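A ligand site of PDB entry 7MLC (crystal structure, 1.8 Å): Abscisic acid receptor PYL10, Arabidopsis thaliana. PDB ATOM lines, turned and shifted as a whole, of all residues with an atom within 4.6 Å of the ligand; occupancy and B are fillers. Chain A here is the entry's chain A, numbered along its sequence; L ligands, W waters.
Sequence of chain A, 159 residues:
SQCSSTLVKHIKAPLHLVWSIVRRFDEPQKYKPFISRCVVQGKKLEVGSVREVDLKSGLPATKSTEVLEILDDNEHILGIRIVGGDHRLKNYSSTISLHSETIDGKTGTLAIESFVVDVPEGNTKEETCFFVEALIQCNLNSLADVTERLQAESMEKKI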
ATOM      1  N   LYS A  32       0.828 -22.828  23.792  1.00  0.00           N
ATOM      2  CA  LYS A  32       1.825 -21.789  23.964  1.00  0.00           C
ATOM      3  C   LYS A  32       2.529 -21.560  22.626  1.00  0.00           C
ATOM      4  O   LYS A  32       3.288 -22.427  22.177  1.00  0.00           O
ATOM      5  CB  LYS A  32       2.816 -22.176  25.047  1.00  0.00           C
ATOM      6  CG  LYS A  32       2.112 -22.312  26.412  1.00  0.00           C
ATOM      7  CD  LYS A  32       3.057 -22.506  27.577  1.00  0.00           C
ATOM      8  CE  LYS A  32       2.277 -22.389  28.885  1.00  0.00           C
ATOM      9  NZ  LYS A  32       3.168 -22.483  30.083  1.00  0.00           N
ATOM     10  N   PHE A  34       5.013 -19.989  21.338  1.00  0.00           N
ATOM     11  CA  PHE A  34       6.444 -19.909  21.106  1.00  0.00           C
ATOM     12  C   PHE A  34       7.169 -21.230  21.365  1.00  0.00           C
ATOM     13  O   PHE A  34       8.394 -21.287  21.216  1.00  0.00           O
ATOM     14  CB  PHE A  34       7.038 -18.786  21.961  1.00  0.00           C
ATOM     15  CG  PHE A  34       6.611 -17.424  21.503  1.00  0.00           C
ATOM     16  CD1 PHE A  34       7.081 -16.913  20.314  1.00  0.00           C
ATOM     17  CD2 PHE A  34       5.714 -16.682  22.246  1.00  0.00           C
ATOM     18  CE1 PHE A  34       6.695 -15.664  19.875  1.00  0.00           C
ATOM     19  CE2 PHE A  34       5.317 -15.428  21.812  1.00  0.00           C
ATOM     20  CZ  PHE A  34       5.808 -14.926  20.627  1.00  0.00           C
ATOM     21  N   ILE A  35       6.431 -22.281  21.695  1.00  0.00           N
ATOM     22  CA  ILE A  35       7.013 -23.579  22.010  1.00  0.00           C
ATOM     23  C   ILE A  35       6.745 -24.538  20.857  1.00  0.00           C
ATOM     24  O   ILE A  35       5.631 -24.589  20.316  1.00  0.00           O
ATOM     25  CB  ILE A  35       6.436 -24.134  23.331  1.00  0.00           C
ATOM     26  CG1 ILE A  35       6.882 -23.245  24.492  1.00  0.00           C
ATOM     27  CG2 ILE A  35       6.864 -25.572  23.520  1.00  0.00           C
ATOM     28  CD1 ILE A  35       6.185 -23.541  25.785  1.00  0.00           C
ATOM     29  N   LEU A  55      12.035 -24.467  21.980  1.00  0.00           N
ATOM     30  CA  LEU A  55      11.358 -23.279  21.497  1.00  0.00           C
ATOM     31  C   LEU A  55      11.308 -23.286  19.976  1.00  0.00           C
ATOM     32  O   LEU A  55      12.068 -23.993  19.309  1.00  0.00           O
ATOM     33  CB  LEU A  55      12.064 -22.019  21.995  1.00  0.00           C
ATOM     34  CG  LEU A  55      12.147 -21.867  23.517  1.00  0.00           C
ATOM     35  CD1 LEU A  55      12.729 -20.522  23.859  1.00  0.00           C
ATOM     36  CD2 LEU A  55      10.784 -22.039  24.167  1.00  0.00           C
ATOM     37  N   LEU A  59      14.295 -17.682  17.704  1.00  0.00           N
ATOM     38  CA  LEU A  59      14.262 -16.960  18.960  1.00  0.00           C
ATOM     39  C   LEU A  59      15.659 -16.859  19.539  1.00  0.00           C
ATOM     40  O   LEU A  59      16.562 -17.602  19.145  1.00  0.00           O
ATOM     41  CB  LEU A  59      13.332 -17.682  19.951  1.00  0.00           C
ATOM     42  CG  LEU A  59      11.860 -17.551  19.567  1.00  0.00           C
ATOM     43  CD1 LEU A  59      10.979 -18.521  20.341  1.00  0.00           C
ATOM     44  CD2 LEU A  59      11.419 -16.113  19.811  1.00  0.00           C
ATOM     45  N   PRO A  60      15.893 -15.933  20.490  1.00  0.00           N
ATOM     46  CA  PRO A  60      17.232 -15.860  21.087  1.00  0.00           C
ATOM     47  C   PRO A  60      17.612 -17.108  21.888  1.00  0.00           C
ATOM     48  O   PRO A  60      18.768 -17.540  21.827  1.00  0.00           O
ATOM     49  CB  PRO A  60      17.161 -14.593  21.964  1.00  0.00           C
ATOM     50  CG  PRO A  60      15.747 -14.201  22.019  1.00  0.00           C
ATOM     51  CD  PRO A  60      15.037 -14.791  20.862  1.00  0.00           C
ATOM     52  N   ALA A  61      16.677 -17.719  22.604  1.00  0.00           N
ATOM     53  CA  ALA A  61      16.925 -18.999  23.255  1.00  0.00           C
ATOM     54  C   ALA A  61      16.364 -20.133  22.392  1.00  0.00           C
ATOM     55  O   ALA A  61      15.643 -19.925  21.421  1.00  0.00           O
ATOM     56  CB  ALA A  61      16.298 -19.026  24.654  1.00  0.00           C
ATOM     57  N   LYS A  63      15.908 -23.599  24.236  1.00  0.00           N
ATOM     58  CA  LYS A  63      15.432 -24.681  25.079  1.00  0.00           C
ATOM     59  C   LYS A  63      15.252 -24.185  26.501  1.00  0.00           C
ATOM     60  O   LYS A  63      15.939 -23.274  26.959  1.00  0.00           O
ATOM     61  CB  LYS A  63      16.395 -25.871  25.057  1.00  0.00           C
ATOM     62  CG  LYS A  63      17.807 -25.496  25.457  1.00  0.00           C
ATOM     63  CD  LYS A  63      18.825 -26.486  24.906  1.00  0.00           C
ATOM     64  CE  LYS A  63      20.237 -25.959  25.119  1.00  0.00           C
ATOM     65  NZ  LYS A  63      21.287 -26.837  24.544  1.00  0.00           N
ATOM     66  N   SER A  64      14.302 -24.816  27.204  1.00  0.00           N
ATOM     67  CA  SER A  64      14.064 -24.594  28.625  1.00  0.00           C
ATOM     68  C   SER A  64      13.926 -25.953  29.296  1.00  0.00           C
ATOM     69  O   SER A  64      13.404 -26.894  28.693  1.00  0.00           O
ATOM     70  CB  SER A  64      12.790 -23.753  28.857  1.00  0.00           C
ATOM     71  OG  SER A  64      12.692 -23.380  30.219  1.00  0.00           O
ATOM     72  N   ILE A  82      11.268 -23.063  36.210  1.00  0.00           N
ATOM     73  CA  ILE A  82      12.303 -23.211  35.175  1.00  0.00           C
ATOM     74  C   ILE A  82      13.640 -23.384  35.860  1.00  0.00           C
ATOM     75  O   ILE A  82      13.999 -22.589  36.743  1.00  0.00           O
ATOM     76  CB  ILE A  82      12.313 -21.997  34.230  1.00  0.00           C
ATOM     77  CG1 ILE A  82      10.962 -21.847  33.518  1.00  0.00           C
ATOM     78  CG2 ILE A  82      13.453 -22.117  33.211  1.00  0.00           C
ATOM     79  CD1 ILE A  82      10.914 -20.681  32.531  1.00  0.00           C
ATOM     80  N   HIS A  87      18.449 -19.306  28.037  1.00  0.00           N
ATOM     81  CA  HIS A  87      17.736 -18.047  28.182  1.00  0.00           C
ATOM     82  C   HIS A  87      18.249 -17.339  29.436  1.00  0.00           C
ATOM     83  O   HIS A  87      19.120 -17.861  30.143  1.00  0.00           O
ATOM     84  CB  HIS A  87      16.240 -18.309  28.294  1.00  0.00           C
ATOM     85  CG  HIS A  87      15.914 -19.251  29.407  1.00  0.00           C
ATOM     86  ND1 HIS A  87      15.815 -18.844  30.719  1.00  0.00           N
ATOM     87  CD2 HIS A  87      15.749 -20.597  29.412  1.00  0.00           C
ATOM     88  CE1 HIS A  87      15.567 -19.902  31.487  1.00  0.00           C
ATOM     89  NE2 HIS A  87      15.515 -20.963  30.715  1.00  0.00           N
ATOM     90  N   ARG A  88      17.662 -16.178  29.739  1.00  0.00           N
ATOM     91  CA  ARG A  88      18.115 -15.356  30.855  1.00  0.00           C
ATOM     92  C   ARG A  88      17.091 -15.248  31.972  1.00  0.00           C
ATOM     93  O   ARG A  88      17.176 -14.326  32.780  1.00  0.00           O
ATOM     94  CB  ARG A  88      18.494 -13.955  30.362  1.00  0.00           C
ATOM     95  CG  ARG A  88      19.296 -13.949  29.100  1.00  0.00           C
ATOM     96  CD  ARG A  88      19.803 -12.554  28.756  1.00  0.00           C
ATOM     97  NE  ARG A  88      18.788 -11.678  28.182  1.00  0.00           N
ATOM     98  CZ  ARG A  88      18.337 -10.580  28.777  1.00  0.00           C
ATOM     99  NH1 ARG A  88      17.419  -9.824  28.180  1.00  0.00           N
ATOM    100  NH2 ARG A  88      18.817 -10.238  29.955  1.00  0.00           N
ATOM    101  N   LEU A  89      16.116 -16.154  32.033  1.00  0.00           N
ATOM    102  CA  LEU A  89      15.157 -16.163  33.129  1.00  0.00           C
ATOM    103  C   LEU A  89      15.728 -17.033  34.250  1.00  0.00           C
ATOM    104  O   LEU A  89      15.860 -18.246  34.083  1.00  0.00           O
ATOM    105  CB  LEU A  89      13.797 -16.666  32.665  1.00  0.00           C
ATOM    106  CG  LEU A  89      13.135 -15.783  31.616  1.00  0.00           C
ATOM    107  CD1 LEU A  89      11.945 -16.494  30.996  1.00  0.00           C
ATOM    108  CD2 LEU A  89      12.700 -14.453  32.221  1.00  0.00           C
ATOM    109  N   TYR A  92      12.662 -18.509  37.777  1.00  0.00           N
ATOM    110  CA  TYR A  92      11.287 -18.312  37.314  1.00  0.00           C
ATOM    111  C   TYR A  92      10.387 -19.422  37.850  1.00  0.00           C
ATOM    112  O   TYR A  92      10.693 -20.604  37.722  1.00  0.00           O
ATOM    113  CB  TYR A  92      11.213 -18.296  35.785  1.00  0.00           C
ATOM    114  CG  TYR A  92       9.798 -18.033  35.283  1.00  0.00           C
ATOM    115  CD1 TYR A  92       8.880 -19.067  35.136  1.00  0.00           C
ATOM    116  CD2 TYR A  92       9.391 -16.740  34.971  1.00  0.00           C
ATOM    117  CE1 TYR A  92       7.596 -18.821  34.691  1.00  0.00           C
ATOM    118  CE2 TYR A  92       8.097 -16.490  34.516  1.00  0.00           C
ATOM    119  CZ  TYR A  92       7.211 -17.538  34.383  1.00  0.00           C
ATOM    120  OH  TYR A  92       5.917 -17.299  33.945  1.00  0.00           O
ATOM    121  N   GLU A 113      -3.060 -16.709  36.514  1.00  0.00           N
ATOM    122  CA  GLU A 113      -1.678 -17.165  36.394  1.00  0.00           C
ATOM    123  C   GLU A 113      -0.748 -16.134  37.044  1.00  0.00           C
ATOM    124  O   GLU A 113      -0.782 -14.947  36.686  1.00  0.00           O
ATOM    125  CB  GLU A 113      -1.309 -17.403  34.921  1.00  0.00           C
ATOM    126  CG  GLU A 113       0.141 -17.854  34.730  1.00  0.00           C
ATOM    127  CD  GLU A 113       0.389 -18.528  33.378  1.00  0.00           C
ATOM    128  OE1 GLU A 113      -0.564 -18.696  32.597  1.00  0.00           O
ATOM    129  OE2 GLU A 113       1.557 -18.913  33.107  1.00  0.00           O
ATOM    130  N   PRO A 120      17.022  -9.903  35.537  1.00  0.00           N
ATOM    131  CA  PRO A 120      18.360 -10.275  35.077  1.00  0.00           C
ATOM    132  C   PRO A 120      19.256  -9.068  34.907  1.00  0.00           C
ATOM    133  O   PRO A 120      18.805  -7.948  34.649  1.00  0.00           O
ATOM    134  CB  PRO A 120      18.096 -10.951  33.728  1.00  0.00           C
ATOM    135  CG  PRO A 120      16.836 -10.330  33.232  1.00  0.00           C
ATOM    136  CD  PRO A 120      16.009 -10.038  34.466  1.00  0.00           C
ATOM    137  N   ASN A 123      18.743  -5.571  32.656  1.00  0.00           N
ATOM    138  CA  ASN A 123      17.363  -5.172  32.460  1.00  0.00           C
ATOM    139  C   ASN A 123      16.833  -4.540  33.745  1.00  0.00           C
ATOM    140  O   ASN A 123      17.319  -4.813  34.847  1.00  0.00           O
ATOM    141  CB  ASN A 123      16.492  -6.368  32.059  1.00  0.00           C
ATOM    142  CG  ASN A 123      16.661  -6.725  30.573  1.00  0.00           C
ATOM    143  OD1 ASN A 123      17.274  -7.742  30.233  1.00  0.00           O
ATOM    144  ND2 ASN A 123      16.131  -5.877  29.701  1.00  0.00           N
ATOM    145  N   GLU A 127      11.147  -3.605  32.755  1.00  0.00           N
ATOM    146  CA  GLU A 127      11.318  -4.359  31.509  1.00  0.00           C
ATOM    147  C   GLU A 127      11.033  -5.836  31.732  1.00  0.00           C
ATOM    148  O   GLU A 127      10.467  -6.513  30.849  1.00  0.00           O
ATOM    149  CB  GLU A 127      12.737  -4.179  30.996  1.00  0.00           C
ATOM    150  CG  GLU A 127      12.986  -2.824  30.355  1.00  0.00           C
ATOM    151  CD  GLU A 127      14.450  -2.466  30.272  1.00  0.00           C
ATOM    152  OE1 GLU A 127      14.745  -1.367  29.772  1.00  0.00           O
ATOM    153  OE2 GLU A 127      15.313  -3.273  30.704  1.00  0.00           O
ATOM    154  N   THR A 128      11.453  -6.368  32.879  1.00  0.00           N
ATOM    155  CA  THR A 128      11.270  -7.777  33.169  1.00  0.00           C
ATOM    156  C   THR A 128       9.793  -8.112  33.340  1.00  0.00           C
ATOM    157  O   THR A 128       9.297  -9.104  32.785  1.00  0.00           O
ATOM    158  CB  THR A 128      12.069  -8.155  34.420  1.00  0.00           C
ATOM    159  OG1 THR A 128      13.441  -7.799  34.230  1.00  0.00           O
ATOM    160  CG2 THR A 128      11.995  -9.641  34.702  1.00  0.00           C
ATOM    161  N   PHE A 131       8.138  -7.947  29.828  1.00  0.00           N
ATOM    162  CA  PHE A 131       8.502  -9.125  29.026  1.00  0.00           C
ATOM    163  C   PHE A 131       7.665 -10.339  29.430  1.00  0.00           C
ATOM    164  O   PHE A 131       7.025 -10.971  28.580  1.00  0.00           O
ATOM    165  CB  PHE A 131       9.995  -9.402  29.178  1.00  0.00           C
ATOM    166  CG  PHE A 131      10.473 -10.636  28.468  1.00  0.00           C
ATOM    167  CD1 PHE A 131      10.738 -10.606  27.106  1.00  0.00           C
ATOM    168  CD2 PHE A 131      10.705 -11.806  29.169  1.00  0.00           C
ATOM    169  CE1 PHE A 131      11.192 -11.746  26.447  1.00  0.00           C
ATOM    170  CE2 PHE A 131      11.159 -12.946  28.510  1.00  0.00           C
ATOM    171  CZ  PHE A 131      11.402 -12.912  27.152  1.00  0.00           C
ATOM    172  N   VAL A 132       7.643 -10.678  30.721  1.00  0.00           N
ATOM    173  CA  VAL A 132       6.938 -11.889  31.135  1.00  0.00           C
ATOM    174  C   VAL A 132       5.432 -11.702  30.983  1.00  0.00           C
ATOM    175  O   VAL A 132       4.733 -12.595  30.513  1.00  0.00           O
ATOM    176  CB  VAL A 132       7.321 -12.280  32.571  1.00  0.00           C
ATOM    177  CG1 VAL A 132       6.523 -13.501  33.018  1.00  0.00           C
ATOM    178  CG2 VAL A 132       8.811 -12.521  32.688  1.00  0.00           C
ATOM    179  N   LEU A 135       4.179 -12.156  27.428  1.00  0.00           N
ATOM    180  CA  LEU A 135       4.212 -13.548  26.975  1.00  0.00           C
ATOM    181  C   LEU A 135       3.120 -14.373  27.636  1.00  0.00           C
ATOM    182  O   LEU A 135       2.488 -15.198  26.982  1.00  0.00           O
ATOM    183  CB  LEU A 135       5.587 -14.161  27.231  1.00  0.00           C
ATOM    184  CG  LEU A 135       6.682 -13.591  26.327  1.00  0.00           C
ATOM    185  CD1 LEU A 135       8.047 -14.047  26.784  1.00  0.00           C
ATOM    186  CD2 LEU A 135       6.431 -13.959  24.858  1.00  0.00           C
ATOM    187  N   ILE A 136       2.897 -14.166  28.938  1.00  0.00           N
ATOM    188  CA  ILE A 136       1.803 -14.876  29.593  1.00  0.00           C
ATOM    189  C   ILE A 136       0.467 -14.448  29.006  1.00  0.00           C
ATOM    190  O   ILE A 136      -0.420 -15.279  28.753  1.00  0.00           O
ATOM    191  CB  ILE A 136       1.838 -14.688  31.115  1.00  0.00           C
ATOM    192  CG1 ILE A 136       3.128 -15.294  31.692  1.00  0.00           C
ATOM    193  CG2 ILE A 136       0.609 -15.334  31.768  1.00  0.00           C
ATOM    194  CD1 ILE A 136       3.196 -15.213  33.202  1.00  0.00           C
ATOM    195  N   ASN A 139       0.020 -16.300  25.874  1.00  0.00           N
ATOM    196  CA  ASN A 139      -0.347 -17.688  26.134  1.00  0.00           C
ATOM    197  C   ASN A 139      -1.804 -17.806  26.595  1.00  0.00           C
ATOM    198  O   ASN A 139      -2.524 -18.712  26.154  1.00  0.00           O
ATOM    199  CB  ASN A 139       0.577 -18.297  27.191  1.00  0.00           C
ATOM    200  CG  ASN A 139       1.987 -18.531  26.664  1.00  0.00           C
ATOM    201  OD1 ASN A 139       2.205 -18.659  25.463  1.00  0.00           O
ATOM    202  ND2 ASN A 139       2.958 -18.574  27.581  1.00  0.00           N
HETATM  203  C1  LIG L   1      13.971  -9.349  30.981  1.00  0.00           C
HETATM  204  C2  LIG L   1      13.625  -8.179  30.307  1.00  0.00           C
HETATM  205  C3  LIG L   1      13.597  -8.161  28.922  1.00  0.00           C
HETATM  206  C4  LIG L   1      13.905  -9.299  28.185  1.00  0.00           C
HETATM  207  C5  LIG L   1      14.244 -10.474  28.844  1.00  0.00           C
HETATM  208  C6  LIG L   1      14.270 -10.489  30.243  1.00  0.00           C
HETATM  209  C7  LIG L   1      14.870 -12.731  28.767  1.00  0.00           C
HETATM  210  C8  LIG L   1      14.912 -12.768  30.150  1.00  0.00           C
HETATM  211  C9  LIG L   1      15.191 -13.886  28.042  1.00  0.00           C
HETATM  212  C10 LIG L   1      15.573 -14.792  25.808  1.00  0.00           C
HETATM  213  C11 LIG L   1      14.413 -15.736  25.452  1.00  0.00           C
HETATM  214  C12 LIG L   1      13.367 -16.066  26.203  1.00  0.00           C
HETATM  215  C13 LIG L   1      11.525 -17.600  25.629  1.00  0.00           C
HETATM  216  C14 LIG L   1      10.418 -17.286  24.826  1.00  0.00           C
HETATM  217  C15 LIG L   1      11.414 -18.622  26.597  1.00  0.00           C
HETATM  218  C16 LIG L   1      10.214 -19.320  26.756  1.00  0.00           C
HETATM  219  C17 LIG L   1       9.104 -18.998  25.959  1.00  0.00           C
HETATM  220  C18 LIG L   1       9.221 -18.004  24.996  1.00  0.00           C
HETATM  221  C19 LIG L   1      10.518 -16.295  23.825  1.00  0.00           C
HETATM  222  C20 LIG L   1      10.410 -14.851  24.208  1.00  0.00           C
HETATM  223  C21 LIG L   1       9.276 -15.509  23.440  1.00  0.00           C
HETATM  224  C22 LIG L   1      12.540 -18.926  27.393  1.00  0.00           C
HETATM  225  C23 LIG L   1      12.859 -20.389  27.594  1.00  0.00           C
HETATM  226  C24 LIG L   1      12.284 -19.570  28.752  1.00  0.00           C
HETATM  227  C25 LIG L   1       7.880 -19.699  26.057  1.00  0.00           C
HETATM  228  C26 LIG L   1       6.922 -19.363  27.192  1.00  0.00           C
HETATM  229  C27 LIG L   1       6.683 -19.044  29.654  1.00  0.00           C
HETATM  230  C28 LIG L   1       7.064 -16.559  29.660  1.00  0.00           C
HETATM  231  C29 LIG L   1       6.025 -17.664  29.625  1.00  0.00           C
HETATM  232  C30 LIG L   1       7.587 -19.162  30.872  1.00  0.00           C
HETATM  233  C31 LIG L   1       8.637 -18.051  30.886  1.00  0.00           C
HETATM  234  C32 LIG L   1       7.929 -16.701  30.899  1.00  0.00           C
HETATM  235  C33 LIG L   1       5.629 -20.161  29.793  1.00  0.00           C
HETATM  236  N1  LIG L   1      14.601 -11.617  30.885  1.00  0.00           N
HETATM  237  N2  LIG L   1      14.552 -11.580  28.152  1.00  0.00           N
HETATM  238  N3  LIG L   1      15.198 -13.717  26.722  1.00  0.00           N
HETATM  239  N4  LIG L   1      13.385 -17.045  24.280  1.00  0.00           N
HETATM  240  N5  LIG L   1      14.338 -16.371  24.281  1.00  0.00           N
HETATM  241  N6  LIG L   1      12.682 -16.930  25.440  1.00  0.00           N
HETATM  242  N7  LIG L   1       7.469 -19.285  28.420  1.00  0.00           N
HETATM  243  O1  LIG L   1      15.468 -14.954  28.593  1.00  0.00           O
HETATM  244  O2  LIG L   1       5.708 -19.272  26.966  1.00  0.00           O
HETATM  245  O3  LIG L   1       4.553 -19.876  30.356  1.00  0.00           O
HETATM  246  O4  LIG L   1       5.944 -21.291  29.374  1.00  0.00           O
HETATM  247  O   HOH W   1       6.521 -22.682  31.447  1.00  0.00           O
HETATM  248  O   HOH W   2       4.620 -19.286  24.268  1.00  0.00           O
HETATM  249  O   HOH W   3       2.042 -18.958  30.411  1.00  0.00           O
HETATM  250  O   HOH W   4      15.934 -11.350  24.854  1.00  0.00           O
HETATM  251  O   HOH W   5       8.961 -22.075  28.609  1.00  0.00           O
HETATM  252  O   HOH W   6       6.598 -24.001  28.992  1.00  0.00           O
HETATM  253  O   HOH W   7       4.263 -19.102  33.148  1.00  0.00           O
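N of Arg 88 is in hydrogen-bond range of O1 of the ligand.
The guanidinium group (NH1) of Arg 88 sits close to a nitrogen (N2) of the ligand (3.4 Å).
ND2 of Asn 139 lies within hydrogen-bond range of O2 of the ligand (2.9 Å).
The side-chain amino group of Lys 32 is in salt-bridge range of an oxygen (O3) of the ligand (3.0 Å).
N5 of the ligand sits at hydrogen-bond distance from N of Ala 61 (3.2 Å).
The guanidinium group of Arg 88 sits at hydrogen-bond distance from the side-chain amide oxygen of Asn 123, 2.9 Å away.
The side-chain amide nitrogen (ND2) of Asn 139 sits close to the backbone carbonyl oxygen (O) of Leu 135 (3.5 Å).
OE2 of Glu 127 lies within hydrogen-bond range of ND2 of Asn 123 (2.9 Å).
A ring nitrogen (ND1) of His 87 sits at hydrogen-bond distance from the backbone NH (N) of Leu 89, at 3.0 Å.
The backbone carbonyl oxygen (O) of Tyr 92 sits at hydrogen-bond distance from the backbone NH (N) of Ile 82 (2.9 Å).
Phe 34 touches the ligand.
CD1 of Leu 55 touches N4 of the ligand (3.6 Å).
Pro 60 touches the ligand (CG to N5, 3.4 Å).
CB of Ser 64 touches C23 of the ligand (3.6 Å).
Ile 82 touches the ligand.
CD2 of His 87 touches C23 of the ligand, 3.4 Å away.
Leu 89 touches the ligand (CD2 to C8, 3.5 Å).
CE2 of Tyr 92 touches C32 of the ligand, 3.6 Å away.
Pro 120 touches the ligand.
Asn 123 touches the ligand (CG to C2, 3.4 Å).
O of Glu 127 touches C2 of the ligand, at 3.6 Å.
Thr 128 touches the ligand (OG1 to C1, 3.6 Å).
Phe 131 touches the ligand (CZ to N2, 3.6 Å).
Leu 135 touches the ligand.
Hydrophobic or aromatic side chains within 4 Å of the ligand: Phe 34, Leu 55, Pro 60, Ala 61, Ile 82, His 87, Leu 89, Tyr 92, Pro 120, Phe 131 and Leu 135.
The nearest printed residue that does not touch the ligand is Ile 35 (4.002 Å).
Water W3 lies within hydrogen-bond range of an oxygen (O3) of the ligand (2.7 Å), the side-chain carboxylate (OE2) of Glu 113 (2.7 Å) and the side-chain amide nitrogen (ND2) of Asn 139 (3.0 Å).
Water W2 lies within hydrogen-bond range of OD1 of Asn 139 (2.8 Å), O2 of the ligand (2.9 Å) and N of Phe 34 (3.0 Å).
Water W7 lies within hydrogen-bond range of OH of Tyr 92 (2.6 Å), OE2 of Glu 113 (2.7 Å) and O3 of the ligand (2.9 Å).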
